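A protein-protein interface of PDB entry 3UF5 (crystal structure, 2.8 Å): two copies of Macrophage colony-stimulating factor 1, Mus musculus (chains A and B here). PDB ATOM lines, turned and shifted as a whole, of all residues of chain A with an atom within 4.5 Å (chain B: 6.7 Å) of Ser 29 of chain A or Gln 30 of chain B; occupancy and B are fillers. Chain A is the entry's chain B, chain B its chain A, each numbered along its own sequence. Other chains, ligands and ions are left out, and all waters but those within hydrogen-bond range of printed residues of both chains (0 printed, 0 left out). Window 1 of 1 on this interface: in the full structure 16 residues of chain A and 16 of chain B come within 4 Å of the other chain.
Ser 29 of chain A touches just these residues of chain B: Ser 29, Gln 30, Phe 71 and Asn 77.
Of the printed residues of chain A, Ser 29 of chain B touches Ser 29 (3.6 Å), Gln 30 (2.6 Å), Phe 71 (3.5 Å) and Asn 77 (2.8 Å).
Printed residues of chain A within 4 Å of Met 31 of chain B: Gln 30 (3.1 Å) and Phe 71 (3.2 Å).
Of the printed residues of chain B, Phe 71 of chain A touches Ser 29, Gln 30, Met 31 and Glu 32.
Of the printed residues of chain B, Asp 28 of chain A touches Lys 72 (3.1 Å) and Thr 75 (3.3 Å).
Printed residues of chain A within 4 Å of Glu 32 of chain B: Phe 71.
Leu 26 of chain A touches none of the printed residues of chain B.
Thr 33 of chain B touches none of the printed residues of chain A.
The nearest residue of chain B that does not touch Ser 29 of chain A is Thr 75 of chain B (4.4 Å).
The nearest printed residue of chain A that does not touch Gln 30 of chain B is Asn 77 of chain A (4.9 Å).
The nearest printed residue of chain A that does not touch Thr 75 of chain B is Ser 29 of chain A (4.4 Å).
Ser 29 of chain B touches its own counterpart, Ser 29 of chain A.
Ser 29 of chain A touches Phe 71 of chain B, and with the chains exchanged Phe 71 of chain A touches Ser 29 of chain B.
Ser 29 of chain A touches Asn 77 of chain B, and with the chains exchanged Asn 77 of chain A touches Ser 29 of chain B.
Met 31 of chain A touches Phe 71 of chain B, and with the chains exchanged Phe 71 of chain A touches Met 31 of chain B.
Of the 19 pairs that touch across the chains among the printed residues, 14 have their exchanged pair printed and touching as well.
The backbone carbonyl oxygen (O) of Leu 26 of chain B is in hydrogen-bond range of the side-chain hydroxyl (OG) of Ser 29 of chain B (2.9 Å).
The side-chain amide nitrogen of Gln 30 of chain A is in hydrogen-bond range of the side-chain hydroxyl of Ser 29 of chain A (3.4 Å).
OG of Ser 29 of chain B lies within hydrogen-bond range of OD1 of Asn 77 of chain B (3.0 Å).
O of Leu 26 of chain A lies within hydrogen-bond range of OG of Ser 29 of chain A (2.8 Å).
OG of Ser 29 of chain A lies within hydrogen-bond range of ND2 of Asn 77 of chain A (3.1 Å).
Of the 17 printed residues of chain B, 9 touch a printed residue of chain A.
Hydrophobic or aromatic side chains of chain B that line the printed part of chain A: Met 31, Phe 71 and Pro 114.
Of the 9 printed residues of chain A, 7 touch a printed residue of chain B.
Hydrophobic or aromatic side chains of chain A within 4 Å of the printed part of chain B: Ile 27, Met 31 and Phe 71.
Along chain A the printed residues that touch a printed residue of chain B span positions 27 to 77.
Among the printed residues, Asp or Glu carboxylates within 4 Å of a Lys or Arg side-chain nitrogen of the other chain: Asp 28 of chain A with Lys 72 of chain B (3.1 Å).
Among the printed residues, merely in contact across the chains: Phe 71 of chain A with Met 31 of chain B, Ser 29 of chain A with Phe 71 of chain B, Asp 28 of chain A with Thr 75 of chain B, Met 31 of chain A with Phe 71 of chain B, Phe 71 of chain A with Ser 29 of chain B, Ser 29 of chain A with Ser 29 of chain B, Ile 27 of chain A with Lys 72 of chain B, Gln 30 of chain A with Phe 71 of chain B, Gln 30 of chain A with Gln 30 of chain B, Phe 71 of chain A with Glu 32 of chain B, Phe 71 of chain A with Gln 30 of chain B and Met 31 of chain A with Pro 114 of chain B.
O of Ser 29 of chain A lies close to OD1 of Asn 77 of chain B.
The side-chain amide oxygen of Gln 30 of chain A is in hydrogen-bond range of the backbone NH of Met 31 of chain B (3.1 Å).
O of Ser 29 of chain B is in hydrogen-bond range of NE2 of Gln 30 of chain A, 2.6 Å away.
The side-chain amide oxygen (OE1) of Gln 30 of chain B sits close to the backbone NH (N) of Met 31 of chain A, 3.2 Å away.
NE2 of Gln 30 of chain B is in hydrogen-bond range of O of Ser 29 of chain A, at 2.8 Å.
The side-chain amino group (NZ) of Lys 72 of chain B lies within salt-bridge range of the side-chain carboxylate (OD1) of Asp 28 of chain A (3.1 Å).
ND2 of Asn 77 of chain A lies within hydrogen-bond range of O of Ser 29 of chain B, 2.8 Å away.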
ATOM      1  N   GLN A  25      -4.296  -2.388   0.550  1.00  0.00           N
ATOM      2  CA  GLN A  25      -5.712  -2.050   0.625  1.00  0.00           C
ATOM      3  C   GLN A  25      -6.053  -1.085  -0.497  1.00  0.00           C
ATOM      4  O   GLN A  25      -7.095  -1.198  -1.143  1.00  0.00           O
ATOM      5  CB  GLN A  25      -6.042  -1.422   1.978  1.00  0.00           C
ATOM      6  CG  GLN A  25      -5.896  -2.379   3.150  1.00  0.00           C
ATOM      7  CD  GLN A  25      -6.095  -1.695   4.485  1.00  0.00           C
ATOM      8  OE1 GLN A  25      -6.222  -0.472   4.556  1.00  0.00           O
ATOM      9  NE2 GLN A  25      -6.123  -2.482   5.556  1.00  0.00           N
ATOM     10  N   LEU A  26      -5.154  -0.137  -0.725  1.00  0.00           N
ATOM     11  CA  LEU A  26      -5.309   0.825  -1.802  1.00  0.00           C
ATOM     12  C   LEU A  26      -5.385   0.092  -3.138  1.00  0.00           C
ATOM     13  O   LEU A  26      -6.296   0.320  -3.931  1.00  0.00           O
ATOM     14  CB  LEU A  26      -4.137   1.803  -1.785  1.00  0.00           C
ATOM     15  CG  LEU A  26      -4.264   3.047  -2.658  1.00  0.00           C
ATOM     16  CD1 LEU A  26      -3.282   4.108  -2.188  1.00  0.00           C
ATOM     17  CD2 LEU A  26      -4.019   2.705  -4.114  1.00  0.00           C
ATOM     18  N   ILE A  27      -4.428  -0.798  -3.377  1.00  0.00           N
ATOM     19  CA  ILE A  27      -4.405  -1.593  -4.599  1.00  0.00           C
ATOM     20  C   ILE A  27      -5.681  -2.410  -4.763  1.00  0.00           C
ATOM     21  O   ILE A  27      -6.295  -2.408  -5.829  1.00  0.00           O
ATOM     22  CB  ILE A  27      -3.209  -2.557  -4.608  1.00  0.00           C
ATOM     23  CG1 ILE A  27      -1.913  -1.778  -4.828  1.00  0.00           C
ATOM     24  CG2 ILE A  27      -3.378  -3.605  -5.701  1.00  0.00           C
ATOM     25  CD1 ILE A  27      -0.654  -2.584  -4.577  1.00  0.00           C
ATOM     26  N   ASP A  28      -6.070  -3.110  -3.702  1.00  0.00           N
ATOM     27  CA  ASP A  28      -7.226  -3.999  -3.743  1.00  0.00           C
ATOM     28  C   ASP A  28      -8.468  -3.287  -4.281  1.00  0.00           C
ATOM     29  O   ASP A  28      -9.237  -3.859  -5.059  1.00  0.00           O
ATOM     30  CB  ASP A  28      -7.510  -4.563  -2.345  1.00  0.00           C
ATOM     31  CG  ASP A  28      -6.389  -5.460  -1.829  1.00  0.00           C
ATOM     32  OD1 ASP A  28      -5.635  -6.019  -2.656  1.00  0.00           O
ATOM     33  OD2 ASP A  28      -6.271  -5.616  -0.593  1.00  0.00           O
ATOM     34  N   SER A  29      -8.650  -2.032  -3.876  1.00  0.00           N
ATOM     35  CA  SER A  29      -9.859  -1.286  -4.209  1.00  0.00           C
ATOM     36  C   SER A  29      -9.905  -0.837  -5.669  1.00  0.00           C
ATOM     37  O   SER A  29     -10.972  -0.502  -6.184  1.00  0.00           O
ATOM     38  CB  SER A  29      -9.994  -0.064  -3.296  1.00  0.00           C
ATOM     39  OG  SER A  29      -8.995   0.902  -3.575  1.00  0.00           O
ATOM     40  N   GLN A  30      -8.755  -0.832  -6.335  1.00  0.00           N
ATOM     41  CA  GLN A  30      -8.676  -0.339  -7.707  1.00  0.00           C
ATOM     42  C   GLN A  30      -9.348  -1.276  -8.708  1.00  0.00           C
ATOM     43  O   GLN A  30      -9.234  -2.497  -8.609  1.00  0.00           O
ATOM     44  CB  GLN A  30      -7.219  -0.108  -8.103  1.00  0.00           C
ATOM     45  CG  GLN A  30      -6.559   1.009  -7.331  1.00  0.00           C
ATOM     46  CD  GLN A  30      -7.342   2.304  -7.409  1.00  0.00           C
ATOM     47  OE1 GLN A  30      -7.455   2.910  -8.476  1.00  0.00           O
ATOM     48  NE2 GLN A  30      -7.896   2.731  -6.279  1.00  0.00           N
ATOM     49  N   MET A  31     -10.043  -0.684  -9.674  1.00  0.00           N
ATOM     50  CA  MET A  31     -10.787  -1.440 -10.675  1.00  0.00           C
ATOM     51  C   MET A  31      -9.884  -1.835 -11.837  1.00  0.00           C
ATOM     52  O   MET A  31      -9.095  -1.027 -12.326  1.00  0.00           O
ATOM     53  CB  MET A  31     -11.957  -0.602 -11.196  1.00  0.00           C
ATOM     54  CG  MET A  31     -12.957  -1.382 -12.039  1.00  0.00           C
ATOM     55  SD  MET A  31     -14.286  -0.348 -12.694  1.00  0.00           S
ATOM     56  CE  MET A  31     -13.424   0.521 -13.998  1.00  0.00           C
ATOM     57  N   PHE A  71      -6.338  11.034  -5.347  1.00  0.00           N
ATOM     58  CA  PHE A  71      -7.571  10.492  -4.791  1.00  0.00           C
ATOM     59  C   PHE A  71      -8.435  11.606  -4.212  1.00  0.00           C
ATOM     60  O   PHE A  71      -7.928  12.643  -3.785  1.00  0.00           O
ATOM     61  CB  PHE A  71      -7.264   9.450  -3.712  1.00  0.00           C
ATOM     62  CG  PHE A  71      -6.623   8.201  -4.243  1.00  0.00           C
ATOM     63  CD1 PHE A  71      -7.390   7.213  -4.833  1.00  0.00           C
ATOM     64  CD2 PHE A  71      -5.253   8.018  -4.159  1.00  0.00           C
ATOM     65  CE1 PHE A  71      -6.806   6.063  -5.327  1.00  0.00           C
ATOM     66  CE2 PHE A  71      -4.661   6.869  -4.652  1.00  0.00           C
ATOM     67  CZ  PHE A  71      -5.439   5.892  -5.236  1.00  0.00           C
ATOM     68  N   ASN A  77      -8.096   6.147   0.837  1.00  0.00           N
ATOM     69  CA  ASN A  77      -6.953   6.037  -0.063  1.00  0.00           C
ATOM     70  C   ASN A  77      -6.147   7.330  -0.112  1.00  0.00           C
ATOM     71  O   ASN A  77      -4.917   7.302  -0.106  1.00  0.00           O
ATOM     72  CB  ASN A  77      -7.411   5.641  -1.468  1.00  0.00           C
ATOM     73  CG  ASN A  77      -7.918   4.209  -1.531  1.00  0.00           C
ATOM     74  OD1 ASN A  77      -8.047   3.539  -0.506  1.00  0.00           O
ATOM     75  ND2 ASN A  77      -8.212   3.736  -2.737  1.00  0.00           N
ATOM     76  N   GLN B  25     -18.882   4.656  -2.299  1.00  0.00           N
ATOM     77  CA  GLN B  25     -17.602   4.223  -1.745  1.00  0.00           C
ATOM     78  C   GLN B  25     -16.719   3.687  -2.863  1.00  0.00           C
ATOM     79  O   GLN B  25     -15.591   4.144  -3.056  1.00  0.00           O
ATOM     80  CB  GLN B  25     -17.808   3.137  -0.690  1.00  0.00           C
ATOM     81  CG  GLN B  25     -18.505   3.619   0.571  1.00  0.00           C
ATOM     82  CD  GLN B  25     -18.775   2.490   1.546  1.00  0.00           C
ATOM     83  OE1 GLN B  25     -18.227   1.395   1.411  1.00  0.00           O
ATOM     84  NE2 GLN B  25     -19.629   2.748   2.531  1.00  0.00           N
ATOM     85  N   LEU B  26     -17.246   2.713  -3.597  1.00  0.00           N
ATOM     86  CA  LEU B  26     -16.543   2.151  -4.739  1.00  0.00           C
ATOM     87  C   LEU B  26     -15.953   3.274  -5.585  1.00  0.00           C
ATOM     88  O   LEU B  26     -14.813   3.188  -6.037  1.00  0.00           O
ATOM     89  CB  LEU B  26     -17.504   1.295  -5.569  1.00  0.00           C
ATOM     90  CG  LEU B  26     -16.940   0.569  -6.792  1.00  0.00           C
ATOM     91  CD1 LEU B  26     -17.829  -0.612  -7.152  1.00  0.00           C
ATOM     92  CD2 LEU B  26     -16.809   1.507  -7.987  1.00  0.00           C
ATOM     93  N   ILE B  27     -16.731   4.333  -5.784  1.00  0.00           N
ATOM     94  CA  ILE B  27     -16.295   5.475  -6.582  1.00  0.00           C
ATOM     95  C   ILE B  27     -15.170   6.246  -5.901  1.00  0.00           C
ATOM     96  O   ILE B  27     -14.193   6.624  -6.545  1.00  0.00           O
ATOM     97  CB  ILE B  27     -17.467   6.446  -6.853  1.00  0.00           C
ATOM     98  CG1 ILE B  27     -18.410   5.860  -7.906  1.00  0.00           C
ATOM     99  CG2 ILE B  27     -16.947   7.802  -7.317  1.00  0.00           C
ATOM    100  CD1 ILE B  27     -19.661   6.686  -8.139  1.00  0.00           C
ATOM    101  N   ASP B  28     -15.311   6.483  -4.602  1.00  0.00           N
ATOM    102  CA  ASP B  28     -14.346   7.297  -3.871  1.00  0.00           C
ATOM    103  C   ASP B  28     -12.973   6.639  -3.780  1.00  0.00           C
ATOM    104  O   ASP B  28     -11.966   7.319  -3.588  1.00  0.00           O
ATOM    105  CB  ASP B  28     -14.866   7.603  -2.465  1.00  0.00           C
ATOM    106  CG  ASP B  28     -16.125   8.454  -2.480  1.00  0.00           C
ATOM    107  OD1 ASP B  28     -16.323   9.217  -3.450  1.00  0.00           O
ATOM    108  OD2 ASP B  28     -16.918   8.356  -1.521  1.00  0.00           O
ATOM    109  N   SER B  29     -12.932   5.319  -3.923  1.00  0.00           N
ATOM    110  CA  SER B  29     -11.681   4.581  -3.778  1.00  0.00           C
ATOM    111  C   SER B  29     -10.874   4.538  -5.078  1.00  0.00           C
ATOM    112  O   SER B  29      -9.718   4.111  -5.080  1.00  0.00           O
ATOM    113  CB  SER B  29     -11.958   3.154  -3.283  1.00  0.00           C
ATOM    114  OG  SER B  29     -12.609   2.370  -4.270  1.00  0.00           O
ATOM    115  N   GLN B  30     -11.474   4.987  -6.178  1.00  0.00           N
ATOM    116  CA  GLN B  30     -10.820   4.908  -7.480  1.00  0.00           C
ATOM    117  C   GLN B  30      -9.848   6.061  -7.707  1.00  0.00           C
ATOM    118  O   GLN B  30     -10.201   7.229  -7.547  1.00  0.00           O
ATOM    119  CB  GLN B  30     -11.859   4.882  -8.599  1.00  0.00           C
ATOM    120  CG  GLN B  30     -12.752   3.658  -8.573  1.00  0.00           C
ATOM    121  CD  GLN B  30     -11.990   2.373  -8.816  1.00  0.00           C
ATOM    122  OE1 GLN B  30     -11.535   2.106  -9.929  1.00  0.00           O
ATOM    123  NE2 GLN B  30     -11.846   1.568  -7.771  1.00  0.00           N
ATOM    124  N   MET B  31      -8.621   5.719  -8.085  1.00  0.00           N
ATOM    125  CA  MET B  31      -7.588   6.715  -8.337  1.00  0.00           C
ATOM    126  C   MET B  31      -7.958   7.567  -9.549  1.00  0.00           C
ATOM    127  O   MET B  31      -8.307   7.043 -10.608  1.00  0.00           O
ATOM    128  CB  MET B  31      -6.237   6.031  -8.568  1.00  0.00           C
ATOM    129  CG  MET B  31      -5.055   6.988  -8.577  1.00  0.00           C
ATOM    130  SD  MET B  31      -3.459   6.154  -8.711  1.00  0.00           S
ATOM    131  CE  MET B  31      -3.542   5.523 -10.386  1.00  0.00           C
ATOM    132  N   GLU B  32      -7.885   8.884  -9.385  1.00  0.00           N
ATOM    133  CA  GLU B  32      -8.201   9.809 -10.468  1.00  0.00           C
ATOM    134  C   GLU B  32      -7.080   9.799 -11.499  1.00  0.00           C
ATOM    135  O   GLU B  32      -5.918  10.048 -11.174  1.00  0.00           O
ATOM    136  CB  GLU B  32      -8.414  11.226  -9.925  1.00  0.00           C
ATOM    137  CG  GLU B  32      -9.339  11.281  -8.713  1.00  0.00           C
ATOM    138  CD  GLU B  32      -9.812  12.687  -8.379  1.00  0.00           C
ATOM    139  OE1 GLU B  32      -9.181  13.336  -7.515  1.00  0.00           O
ATOM    140  OE2 GLU B  32     -10.819  13.138  -8.969  1.00  0.00           O
ATOM    141  N   THR B  33      -7.433   9.497 -12.743  1.00  0.00           N
ATOM    142  CA  THR B  33      -6.464   9.490 -13.829  1.00  0.00           C
ATOM    143  C   THR B  33      -7.125   9.999 -15.101  1.00  0.00           C
ATOM    144  O   THR B  33      -8.345  10.165 -15.150  1.00  0.00           O
ATOM    145  CB  THR B  33      -5.914   8.076 -14.083  1.00  0.00           C
ATOM    146  OG1 THR B  33      -6.906   7.282 -14.748  1.00  0.00           O
ATOM    147  CG2 THR B  33      -5.524   7.411 -12.771  1.00  0.00           C
ATOM    148  N   PHE B  71     -13.253  -6.471 -10.177  1.00  0.00           N
ATOM    149  CA  PHE B  71     -12.412  -6.284  -9.000  1.00  0.00           C
ATOM    150  C   PHE B  71     -11.877  -7.628  -8.516  1.00  0.00           C
ATOM    151  O   PHE B  71     -12.423  -8.680  -8.857  1.00  0.00           O
ATOM    152  CB  PHE B  71     -13.201  -5.604  -7.879  1.00  0.00           C
ATOM    153  CG  PHE B  71     -13.632  -4.203  -8.206  1.00  0.00           C
ATOM    154  CD1 PHE B  71     -12.796  -3.127  -7.948  1.00  0.00           C
ATOM    155  CD2 PHE B  71     -14.876  -3.960  -8.770  1.00  0.00           C
ATOM    156  CE1 PHE B  71     -13.191  -1.837  -8.247  1.00  0.00           C
ATOM    157  CE2 PHE B  71     -15.277  -2.670  -9.072  1.00  0.00           C
ATOM    158  CZ  PHE B  71     -14.434  -1.607  -8.809  1.00  0.00           C
ATOM    159  N   LYS B  72     -10.807  -7.590  -7.728  1.00  0.00           N
ATOM    160  CA  LYS B  72     -10.230  -8.810  -7.177  1.00  0.00           C
ATOM    161  C   LYS B  72     -11.215  -9.459  -6.213  1.00  0.00           C
ATOM    162  O   LYS B  72     -11.869  -8.774  -5.429  1.00  0.00           O
ATOM    163  CB  LYS B  72      -8.903  -8.516  -6.473  1.00  0.00           C
ATOM    164  CG  LYS B  72      -7.825  -7.960  -7.396  1.00  0.00           C
ATOM    165  CD  LYS B  72      -6.435  -8.462  -7.014  1.00  0.00           C
ATOM    166  CE  LYS B  72      -5.971  -7.921  -5.667  1.00  0.00           C
ATOM    167  NZ  LYS B  72      -5.648  -6.469  -5.729  1.00  0.00           N
ATOM    168  N   THR B  75     -13.078  -8.743  -2.529  1.00  0.00           N
ATOM    169  CA  THR B  75     -12.703  -7.368  -2.239  1.00  0.00           C
ATOM    170  C   THR B  75     -13.964  -6.553  -1.971  1.00  0.00           C
ATOM    171  O   THR B  75     -14.998  -6.790  -2.595  1.00  0.00           O
ATOM    172  CB  THR B  75     -11.951  -6.751  -3.430  1.00  0.00           C
ATOM    173  OG1 THR B  75     -10.771  -7.517  -3.706  1.00  0.00           O
ATOM    174  CG2 THR B  75     -11.564  -5.312  -3.145  1.00  0.00           C
ATOM    175  N   PRO B  76     -13.889  -5.590  -1.039  1.00  0.00           N
ATOM    176  CA  PRO B  76     -15.046  -4.737  -0.744  1.00  0.00           C
ATOM    177  C   PRO B  76     -15.798  -4.256  -1.991  1.00  0.00           C
ATOM    178  O   PRO B  76     -17.020  -4.393  -2.050  1.00  0.00           O
ATOM    179  CB  PRO B  76     -14.415  -3.559  -0.006  1.00  0.00           C
ATOM    180  CG  PRO B  76     -13.272  -4.172   0.726  1.00  0.00           C
ATOM    181  CD  PRO B  76     -12.745  -5.273  -0.165  1.00  0.00           C
ATOM    182  N   ASN B  77     -15.083  -3.698  -2.965  1.00  0.00           N
ATOM    183  CA  ASN B  77     -15.705  -3.265  -4.215  1.00  0.00           C
ATOM    184  C   ASN B  77     -16.203  -4.447  -5.044  1.00  0.00           C
ATOM    185  O   ASN B  77     -17.213  -4.342  -5.743  1.00  0.00           O
ATOM    186  CB  ASN B  77     -14.734  -2.424  -5.050  1.00  0.00           C
ATOM    187  CG  ASN B  77     -14.303  -1.139  -4.353  1.00  0.00           C
ATOM    188  OD1 ASN B  77     -13.312  -0.520  -4.748  1.00  0.00           O
ATOM    189  ND2 ASN B  77     -15.036  -0.731  -3.315  1.00  0.00           N
ATOM    190  N   PRO B 114     -12.842   6.098 -16.072  1.00  0.00           N
ATOM    191  CA  PRO B 114     -13.677   5.175 -15.295  1.00  0.00           C
ATOM    192  C   PRO B 114     -14.568   5.888 -14.273  1.00  0.00           C
ATOM    193  O   PRO B 114     -15.716   5.484 -14.075  1.00  0.00           O
ATOM    194  CB  PRO B 114     -12.648   4.282 -14.594  1.00  0.00           C
ATOM    195  CG  PRO B 114     -11.451   4.331 -15.473  1.00  0.00           C
ATOM    196  CD  PRO B 114     -11.418   5.725 -16.020  1.00  0.00           C
ATOM    197  N   LEU B 115     -14.047   6.931 -13.635  1.00  0.00           N
ATOM    198  CA  LEU B 115     -14.822   7.683 -12.654  1.00  0.00           C
ATOM    199  C   LEU B 115     -16.031   8.352 -13.301  1.00  0.00           C
ATOM    200  O   LEU B 115     -17.113   8.387 -12.718  1.00  0.00           O
ATOM    201  CB  LEU B 115     -13.946   8.729 -11.964  1.00  0.00           C
ATOM    202  CG  LEU B 115     -13.088   8.191 -10.819  1.00  0.00           C
ATOM    203  CD1 LEU B 115     -12.020   9.197 -10.423  1.00  0.00           C
ATOM    204  CD2 LEU B 115     -13.963   7.854  -9.626  1.00  0.00           C
ATOM    205  N   LEU B 118     -18.487   5.724 -13.959  1.00  0.00           N
ATOM    206  CA  LEU B 118     -19.159   5.315 -12.730  1.00  0.00           C
ATOM    207  C   LEU B 118     -20.216   6.334 -12.333  1.00  0.00           C
ATOM    208  O   LEU B 118     -21.294   5.969 -11.868  1.00  0.00           O
ATOM    209  CB  LEU B 118     -18.155   5.133 -11.593  1.00  0.00           C
ATOM    210  CG  LEU B 118     -17.208   3.938 -11.721  1.00  0.00           C
ATOM    211  CD1 LEU B 118     -16.179   3.960 -10.606  1.00  0.00           C
ATOM    212  CD2 LEU B 118     -17.986   2.631 -11.707  1.00  0.00           C
